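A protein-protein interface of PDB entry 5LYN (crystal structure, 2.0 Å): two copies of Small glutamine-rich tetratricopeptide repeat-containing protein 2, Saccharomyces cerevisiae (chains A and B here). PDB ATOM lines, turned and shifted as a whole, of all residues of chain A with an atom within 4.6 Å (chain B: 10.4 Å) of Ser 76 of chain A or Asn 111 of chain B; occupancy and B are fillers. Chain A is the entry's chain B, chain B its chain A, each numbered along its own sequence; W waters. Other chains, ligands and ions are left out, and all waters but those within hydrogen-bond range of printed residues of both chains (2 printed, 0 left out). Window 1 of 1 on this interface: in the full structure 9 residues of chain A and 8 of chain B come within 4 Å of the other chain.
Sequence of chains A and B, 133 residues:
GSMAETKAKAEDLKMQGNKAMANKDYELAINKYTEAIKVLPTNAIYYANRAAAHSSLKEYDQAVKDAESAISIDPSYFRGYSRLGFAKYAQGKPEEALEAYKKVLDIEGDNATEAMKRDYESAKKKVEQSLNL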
ATOM      1  N   ASP A  74      11.909   2.370  11.981  1.00  0.00           N
ATOM      2  CA  ASP A  74      12.841   2.903  10.986  1.00  0.00           C
ATOM      3  C   ASP A  74      13.919   1.869  10.726  1.00  0.00           C
ATOM      4  O   ASP A  74      14.941   1.821  11.427  1.00  0.00           O
ATOM      5  CB  ASP A  74      13.460   4.227  11.435  1.00  0.00           C
ATOM      6  CG  ASP A  74      14.367   4.845  10.359  1.00  0.00           C
ATOM      7  OD1 ASP A  74      14.601   4.197   9.310  1.00  0.00           O
ATOM      8  OD2 ASP A  74      14.858   5.978  10.571  1.00  0.00           O
ATOM      9  N   PRO A  75      13.741   1.044   9.692  1.00  0.00           N
ATOM     10  CA  PRO A  75      14.713  -0.019   9.405  1.00  0.00           C
ATOM     11  C   PRO A  75      16.053   0.486   8.876  1.00  0.00           C
ATOM     12  O   PRO A  75      16.963  -0.332   8.699  1.00  0.00           O
ATOM     13  CB  PRO A  75      14.001  -0.876   8.349  1.00  0.00           C
ATOM     14  CG  PRO A  75      12.583  -0.401   8.309  1.00  0.00           C
ATOM     15  CD  PRO A  75      12.575   1.002   8.796  1.00  0.00           C
ATOM     16  N   SER A  76      16.203   1.776   8.602  1.00  0.00           N
ATOM     17  CA  SER A  76      17.478   2.321   8.158  1.00  0.00           C
ATOM     18  C   SER A  76      18.245   2.991   9.291  1.00  0.00           C
ATOM     19  O   SER A  76      19.373   3.446   9.081  1.00  0.00           O
ATOM     20  CB  SER A  76      17.264   3.322   7.017  1.00  0.00           C
ATOM     21  OG  SER A  76      16.652   4.515   7.484  1.00  0.00           O
ATOM     22  N   TYR A  77      17.652   3.077  10.476  1.00  0.00           N
ATOM     23  CA  TYR A  77      18.335   3.633  11.643  1.00  0.00           C
ATOM     24  C   TYR A  77      19.199   2.520  12.226  1.00  0.00           C
ATOM     25  O   TYR A  77      18.696   1.608  12.885  1.00  0.00           O
ATOM     26  CB  TYR A  77      17.308   4.170  12.636  1.00  0.00           C
ATOM     27  CG  TYR A  77      17.889   4.711  13.920  1.00  0.00           C
ATOM     28  CD1 TYR A  77      18.580   5.921  13.940  1.00  0.00           C
ATOM     29  CD2 TYR A  77      17.729   4.026  15.116  1.00  0.00           C
ATOM     30  CE1 TYR A  77      19.117   6.421  15.114  1.00  0.00           C
ATOM     31  CE2 TYR A  77      18.266   4.520  16.298  1.00  0.00           C
ATOM     32  CZ  TYR A  77      18.955   5.720  16.287  1.00  0.00           C
ATOM     33  OH  TYR A  77      19.480   6.221  17.452  1.00  0.00           O
ATOM     34  N   PHE A  78      20.512   2.550  11.955  1.00  0.00           N
ATOM     35  CA  PHE A  78      21.291   1.352  12.246  1.00  0.00           C
ATOM     36  C   PHE A  78      21.499   1.113  13.739  1.00  0.00           C
ATOM     37  O   PHE A  78      21.731  -0.035  14.130  1.00  0.00           O
ATOM     38  CB  PHE A  78      22.645   1.363  11.508  1.00  0.00           C
ATOM     39  CG  PHE A  78      23.575   2.486  11.900  1.00  0.00           C
ATOM     40  CD1 PHE A  78      24.209   2.493  13.136  1.00  0.00           C
ATOM     41  CD2 PHE A  78      23.864   3.501  10.994  1.00  0.00           C
ATOM     42  CE1 PHE A  78      25.077   3.515  13.478  1.00  0.00           C
ATOM     43  CE2 PHE A  78      24.743   4.522  11.323  1.00  0.00           C
ATOM     44  CZ  PHE A  78      25.344   4.530  12.572  1.00  0.00           C
ATOM     45  N   ARG A  79      21.436   2.144  14.585  1.00  0.00           N
ATOM     46  CA  ARG A  79      21.607   1.887  16.016  1.00  0.00           C
ATOM     47  C   ARG A  79      20.551   0.922  16.553  1.00  0.00           C
ATOM     48  O   ARG A  79      20.797   0.232  17.544  1.00  0.00           O
ATOM     49  CB  ARG A  79      21.568   3.183  16.821  1.00  0.00           C
ATOM     50  CG  ARG A  79      22.901   3.910  16.865  1.00  0.00           C
ATOM     51  CD  ARG A  79      24.026   2.926  17.121  1.00  0.00           C
ATOM     52  NE  ARG A  79      25.312   3.584  17.314  1.00  0.00           N
ATOM     53  CZ  ARG A  79      26.478   2.965  17.182  1.00  0.00           C
ATOM     54  NH1 ARG A  79      27.610   3.629  17.373  1.00  0.00           N
ATOM     55  NH2 ARG A  79      26.505   1.678  16.845  1.00  0.00           N
ATOM     56  N   ILE A 107      24.240  -1.750   6.234  1.00  0.00           N
ATOM     57  CA  ILE A 107      23.713  -0.401   6.058  1.00  0.00           C
ATOM     58  C   ILE A 107      24.854   0.582   5.835  1.00  0.00           C
ATOM     59  O   ILE A 107      24.824   1.397   4.910  1.00  0.00           O
ATOM     60  CB  ILE A 107      22.852  -0.011   7.276  1.00  0.00           C
ATOM     61  CG1 ILE A 107      21.584  -0.852   7.321  1.00  0.00           C
ATOM     62  CG2 ILE A 107      22.521   1.476   7.274  1.00  0.00           C
ATOM     63  CD1 ILE A 107      20.810  -0.682   8.607  1.00  0.00           C
ATOM     64  N   PHE B  78      30.715   9.105   3.502  1.00  0.00           N
ATOM     65  CA  PHE B  78      30.449  10.476   3.921  1.00  0.00           C
ATOM     66  C   PHE B  78      31.693  11.181   4.430  1.00  0.00           C
ATOM     67  O   PHE B  78      31.726  12.409   4.436  1.00  0.00           O
ATOM     68  CB  PHE B  78      29.322  10.552   4.963  1.00  0.00           C
ATOM     69  CG  PHE B  78      29.598   9.829   6.249  1.00  0.00           C
ATOM     70  CD1 PHE B  78      30.528  10.303   7.152  1.00  0.00           C
ATOM     71  CD2 PHE B  78      28.868   8.698   6.579  1.00  0.00           C
ATOM     72  CE1 PHE B  78      30.758   9.638   8.346  1.00  0.00           C
ATOM     73  CE2 PHE B  78      29.084   8.039   7.781  1.00  0.00           C
ATOM     74  CZ  PHE B  78      30.037   8.510   8.657  1.00  0.00           C
ATOM     75  N   VAL B 104      26.843  15.360   4.503  1.00  0.00           N
ATOM     76  CA  VAL B 104      27.024  14.302   5.501  1.00  0.00           C
ATOM     77  C   VAL B 104      25.711  14.029   6.221  1.00  0.00           C
ATOM     78  O   VAL B 104      25.307  12.871   6.401  1.00  0.00           O
ATOM     79  CB  VAL B 104      28.135  14.693   6.498  1.00  0.00           C
ATOM     80  CG1 VAL B 104      28.288  13.625   7.602  1.00  0.00           C
ATOM     81  CG2 VAL B 104      29.452  14.941   5.768  1.00  0.00           C
ATOM     82  N   LEU B 105      25.027  15.094   6.655  1.00  0.00           N
ATOM     83  CA  LEU B 105      23.755  14.930   7.359  1.00  0.00           C
ATOM     84  C   LEU B 105      22.672  14.366   6.450  1.00  0.00           C
ATOM     85  O   LEU B 105      21.786  13.639   6.914  1.00  0.00           O
ATOM     86  CB  LEU B 105      23.296  16.266   7.944  1.00  0.00           C
ATOM     87  CG  LEU B 105      24.194  16.883   9.020  1.00  0.00           C
ATOM     88  CD1 LEU B 105      23.586  18.160   9.566  1.00  0.00           C
ATOM     89  CD2 LEU B 105      24.465  15.923  10.137  1.00  0.00           C
ATOM     90  N   ASP B 106      22.722  14.684   5.155  1.00  0.00           N
ATOM     91  CA  ASP B 106      21.747  14.118   4.234  1.00  0.00           C
ATOM     92  C   ASP B 106      22.007  12.634   3.992  1.00  0.00           C
ATOM     93  O   ASP B 106      21.066  11.843   3.902  1.00  0.00           O
ATOM     94  CB  ASP B 106      21.755  14.904   2.924  1.00  0.00           C
ATOM     95  CG  ASP B 106      21.188  16.309   3.087  1.00  0.00           C
ATOM     96  OD1 ASP B 106      20.382  16.525   4.017  1.00  0.00           O
ATOM     97  OD2 ASP B 106      21.547  17.199   2.282  1.00  0.00           O
ATOM     98  N   ILE B 107      23.275  12.235   3.907  1.00  0.00           N
ATOM     99  CA  ILE B 107      23.606  10.819   3.759  1.00  0.00           C
ATOM    100  C   ILE B 107      23.174  10.039   4.993  1.00  0.00           C
ATOM    101  O   ILE B 107      22.533   8.985   4.891  1.00  0.00           O
ATOM    102  CB  ILE B 107      25.113  10.653   3.500  1.00  0.00           C
ATOM    103  CG1 ILE B 107      25.472  11.127   2.086  1.00  0.00           C
ATOM    104  CG2 ILE B 107      25.559   9.220   3.746  1.00  0.00           C
ATOM    105  CD1 ILE B 107      26.939  11.447   1.952  1.00  0.00           C
ATOM    106  N   GLU B 108      23.529  10.539   6.181  1.00  0.00           N
ATOM    107  CA  GLU B 108      23.288   9.785   7.404  1.00  0.00           C
ATOM    108  C   GLU B 108      21.869   9.948   7.945  1.00  0.00           C
ATOM    109  O   GLU B 108      21.369   9.033   8.605  1.00  0.00           O
ATOM    110  CB  GLU B 108      24.305  10.185   8.473  1.00  0.00           C
ATOM    111  CG  GLU B 108      25.649   9.534   8.275  1.00  0.00           C
ATOM    112  CD  GLU B 108      25.524   8.023   8.091  1.00  0.00           C
ATOM    113  OE1 GLU B 108      25.208   7.332   9.077  1.00  0.00           O
ATOM    114  OE2 GLU B 108      25.719   7.532   6.955  1.00  0.00           O
ATOM    115  N   GLY B 109      21.210  11.081   7.705  1.00  0.00           N
ATOM    116  CA  GLY B 109      19.845  11.229   8.205  1.00  0.00           C
ATOM    117  C   GLY B 109      19.789  11.100   9.716  1.00  0.00           C
ATOM    118  O   GLY B 109      20.643  11.619  10.434  1.00  0.00           O
ATOM    119  N   ASP B 110      18.786  10.361  10.215  1.00  0.00           N
ATOM    120  CA  ASP B 110      18.639  10.155  11.657  1.00  0.00           C
ATOM    121  C   ASP B 110      19.800   9.389  12.281  1.00  0.00           C
ATOM    122  O   ASP B 110      19.874   9.309  13.517  1.00  0.00           O
ATOM    123  CB  ASP B 110      17.340   9.409  11.959  1.00  0.00           C
ATOM    124  CG  ASP B 110      16.112  10.264  11.741  1.00  0.00           C
ATOM    125  OD1 ASP B 110      16.266  11.470  11.449  1.00  0.00           O
ATOM    126  OD2 ASP B 110      14.991   9.735  11.882  1.00  0.00           O
ATOM    127  N   ASN B 111      20.690   8.809  11.472  1.00  0.00           N
ATOM    128  CA  ASN B 111      21.901   8.184  11.987  1.00  0.00           C
ATOM    129  C   ASN B 111      23.004   9.181  12.324  1.00  0.00           C
ATOM    130  O   ASN B 111      24.018   8.781  12.911  1.00  0.00           O
ATOM    131  CB  ASN B 111      22.456   7.188  10.972  1.00  0.00           C
ATOM    132  CG  ASN B 111      21.512   6.058  10.701  1.00  0.00           C
ATOM    133  OD1 ASN B 111      21.110   5.328  11.617  1.00  0.00           O
ATOM    134  ND2 ASN B 111      21.136   5.905   9.440  1.00  0.00           N
ATOM    135  N   ALA B 112      22.849  10.450  11.956  1.00  0.00           N
ATOM    136  CA  ALA B 112      23.942  11.399  12.131  1.00  0.00           C
ATOM    137  C   ALA B 112      24.331  11.520  13.599  1.00  0.00           C
ATOM    138  O   ALA B 112      23.475  11.534  14.486  1.00  0.00           O
ATOM    139  CB  ALA B 112      23.548  12.769  11.575  1.00  0.00           C
ATOM    140  N   THR B 113      25.635  11.599  13.849  1.00  0.00           N
ATOM    141  CA  THR B 113      26.176  11.743  15.192  1.00  0.00           C
ATOM    142  C   THR B 113      26.134  13.206  15.634  1.00  0.00           C
ATOM    143  O   THR B 113      25.913  14.127  14.840  1.00  0.00           O
ATOM    144  CB  THR B 113      27.608  11.226  15.234  1.00  0.00           C
ATOM    145  OG1 THR B 113      28.447  12.113  14.480  1.00  0.00           O
ATOM    146  CG2 THR B 113      27.677   9.831  14.609  1.00  0.00           C
ATOM    147  N   GLU B 114      26.370  13.423  16.926  1.00  0.00           N
ATOM    148  CA  GLU B 114      26.416  14.794  17.416  1.00  0.00           C
ATOM    149  C   GLU B 114      27.620  15.546  16.856  1.00  0.00           C
ATOM    150  O   GLU B 114      27.549  16.761  16.649  1.00  0.00           O
ATOM    151  CB  GLU B 114      26.414  14.805  18.943  1.00  0.00           C
ATOM    152  CG  GLU B 114      25.107  14.280  19.557  1.00  0.00           C
ATOM    153  CD  GLU B 114      23.860  14.903  18.931  1.00  0.00           C
ATOM    154  OE1 GLU B 114      23.028  14.152  18.374  1.00  0.00           O
ATOM    155  OE2 GLU B 114      23.715  16.145  18.988  1.00  0.00           O
ATOM    156  N   ALA B 115      28.716  14.844  16.572  1.00  0.00           N
ATOM    157  CA  ALA B 115      29.849  15.495  15.923  1.00  0.00           C
ATOM    158  C   ALA B 115      29.469  16.026  14.544  1.00  0.00           C
ATOM    159  O   ALA B 115      29.829  17.155  14.187  1.00  0.00           O
ATOM    160  CB  ALA B 115      31.024  14.530  15.823  1.00  0.00           C
ATOM    161  N   MET B 116      28.741  15.232  13.748  1.00  0.00           N
ATOM    162  CA  MET B 116      28.351  15.706  12.422  1.00  0.00           C
ATOM    163  C   MET B 116      27.486  16.958  12.507  1.00  0.00           C
ATOM    164  O   MET B 116      27.630  17.882  11.694  1.00  0.00           O
ATOM    165  CB  MET B 116      27.610  14.613  11.669  1.00  0.00           C
ATOM    166  CG  MET B 116      28.436  13.376  11.390  1.00  0.00           C
ATOM    167  SD  MET B 116      27.346  12.013  10.942  1.00  0.00           S
ATOM    168  CE  MET B 116      28.483  10.634  11.052  1.00  0.00           C
ATOM    169  N   LYS B 117      26.569  17.006  13.475  1.00  0.00           N
ATOM    170  CA  LYS B 117      25.723  18.184  13.602  1.00  0.00           C
ATOM    171  C   LYS B 117      26.510  19.380  14.120  1.00  0.00           C
ATOM    172  O   LYS B 117      26.236  20.515  13.719  1.00  0.00           O
ATOM    173  CB  LYS B 117      24.537  17.894  14.520  1.00  0.00           C
ATOM    174  CG  LYS B 117      23.697  16.691  14.108  1.00  0.00           C
ATOM    175  CD  LYS B 117      22.500  16.584  15.054  1.00  0.00           C
ATOM    176  CE  LYS B 117      21.967  15.173  15.155  1.00  0.00           C
ATOM    177  NZ  LYS B 117      20.902  15.071  16.199  1.00  0.00           N
HETATM  178  O   HOH W   1      14.790   7.461  12.812  1.00  0.00           O
HETATM  179  O   HOH W   2      21.742   5.058  14.212  1.00  0.00           O
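The side-chain carboxylate (OD1) of Asp 74 of chain A lies within hydrogen-bond range of the backbone NH (N) of Tyr 77 of chain A (3.5 Å).
The side-chain amide nitrogen of Asn 111 of chain B sits close to the backbone carbonyl oxygen of Glu 108 of chain B, 3.2 Å away.
The side-chain hydroxyl of Ser 76 of chain A lies within hydrogen-bond range of the side-chain carboxylate of Asp 74 of chain A.
Of the 7 printed residues of chain A, 4 touch a printed residue of chain B.
Printed residues of chain A that touch a printed residue of chain B: Asp 74, Ser 76, Tyr 77 and Phe 78.
Hydrophobic or aromatic side chains of chain A that line the printed part of chain B: Tyr 77 and Phe 78.
Printed residues of chain B that touch a printed residue of chain A: Glu 108, Asp 110 and Asn 111.
Among the printed residues, 6 pairs touch across the chains.
Water W1 lies within hydrogen-bond range of the side-chain carboxylate (OD2) of Asp 110 of chain B (2.5 Å) and the side-chain carboxylate (OD2) of Asp 74 of chain A (2.7 Å).
Water W2 lies within hydrogen-bond range of OD1 of Asn 111 of chain B and N of Arg 79 of chain A.
OD1 of Asn 111 of chain B lies within hydrogen-bond range of N of Phe 78 of chain A (2.9 Å).
The side-chain amide nitrogen (ND2) of Asn 111 of chain B is in hydrogen-bond range of the backbone carbonyl oxygen (O) of Ser 76 of chain A (3.0 Å).
Ser 76 of chain A touches just one residue of chain B: Asn 111.
Asn 111 of chain B touches just these residues of chain A: Ser 76, Tyr 77 and Phe 78.
No residue of chain B comes within 4 Å of Pro 75 of chain A.
Phe 78 of chain A touches just these residues of chain B: Glu 108 and Asn 111.
Printed residues of chain B within 4 Å of Asp 74 of chain A: Asp 110 (3.98 Å).
Of the printed residues of chain A, Glu 108 of chain B touches Phe 78 (3.6 Å).
Printed residues of chain A within 4 Å of Asp 110 of chain B: Asp 74 (3.98 Å) and Tyr 77 (3.4 Å).
The nearest residue of chain B that does not touch Ser 76 of chain A is Glu 108 of chain B (6.0 Å).
The nearest residue of chain A that does not touch Asn 111 of chain B is Arg 79 of chain A (4.4 Å).
Positions printed for both chains: 78 and 107.
Of the 6 pairs that touch across the chains among the printed residues, none has its exchanged pair printed and touching as well.
Among the printed residues, pairs that only touch across the chains: Tyr 77 of chain A with Asn 111 of chain B (3.3 Å), Tyr 77 of chain A with Asp 110 of chain B (3.4 Å), Phe 78 of chain A with Glu 108 of chain B (3.6 Å) and Asp 74 of chain A with Asp 110 of chain B (3.98 Å).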
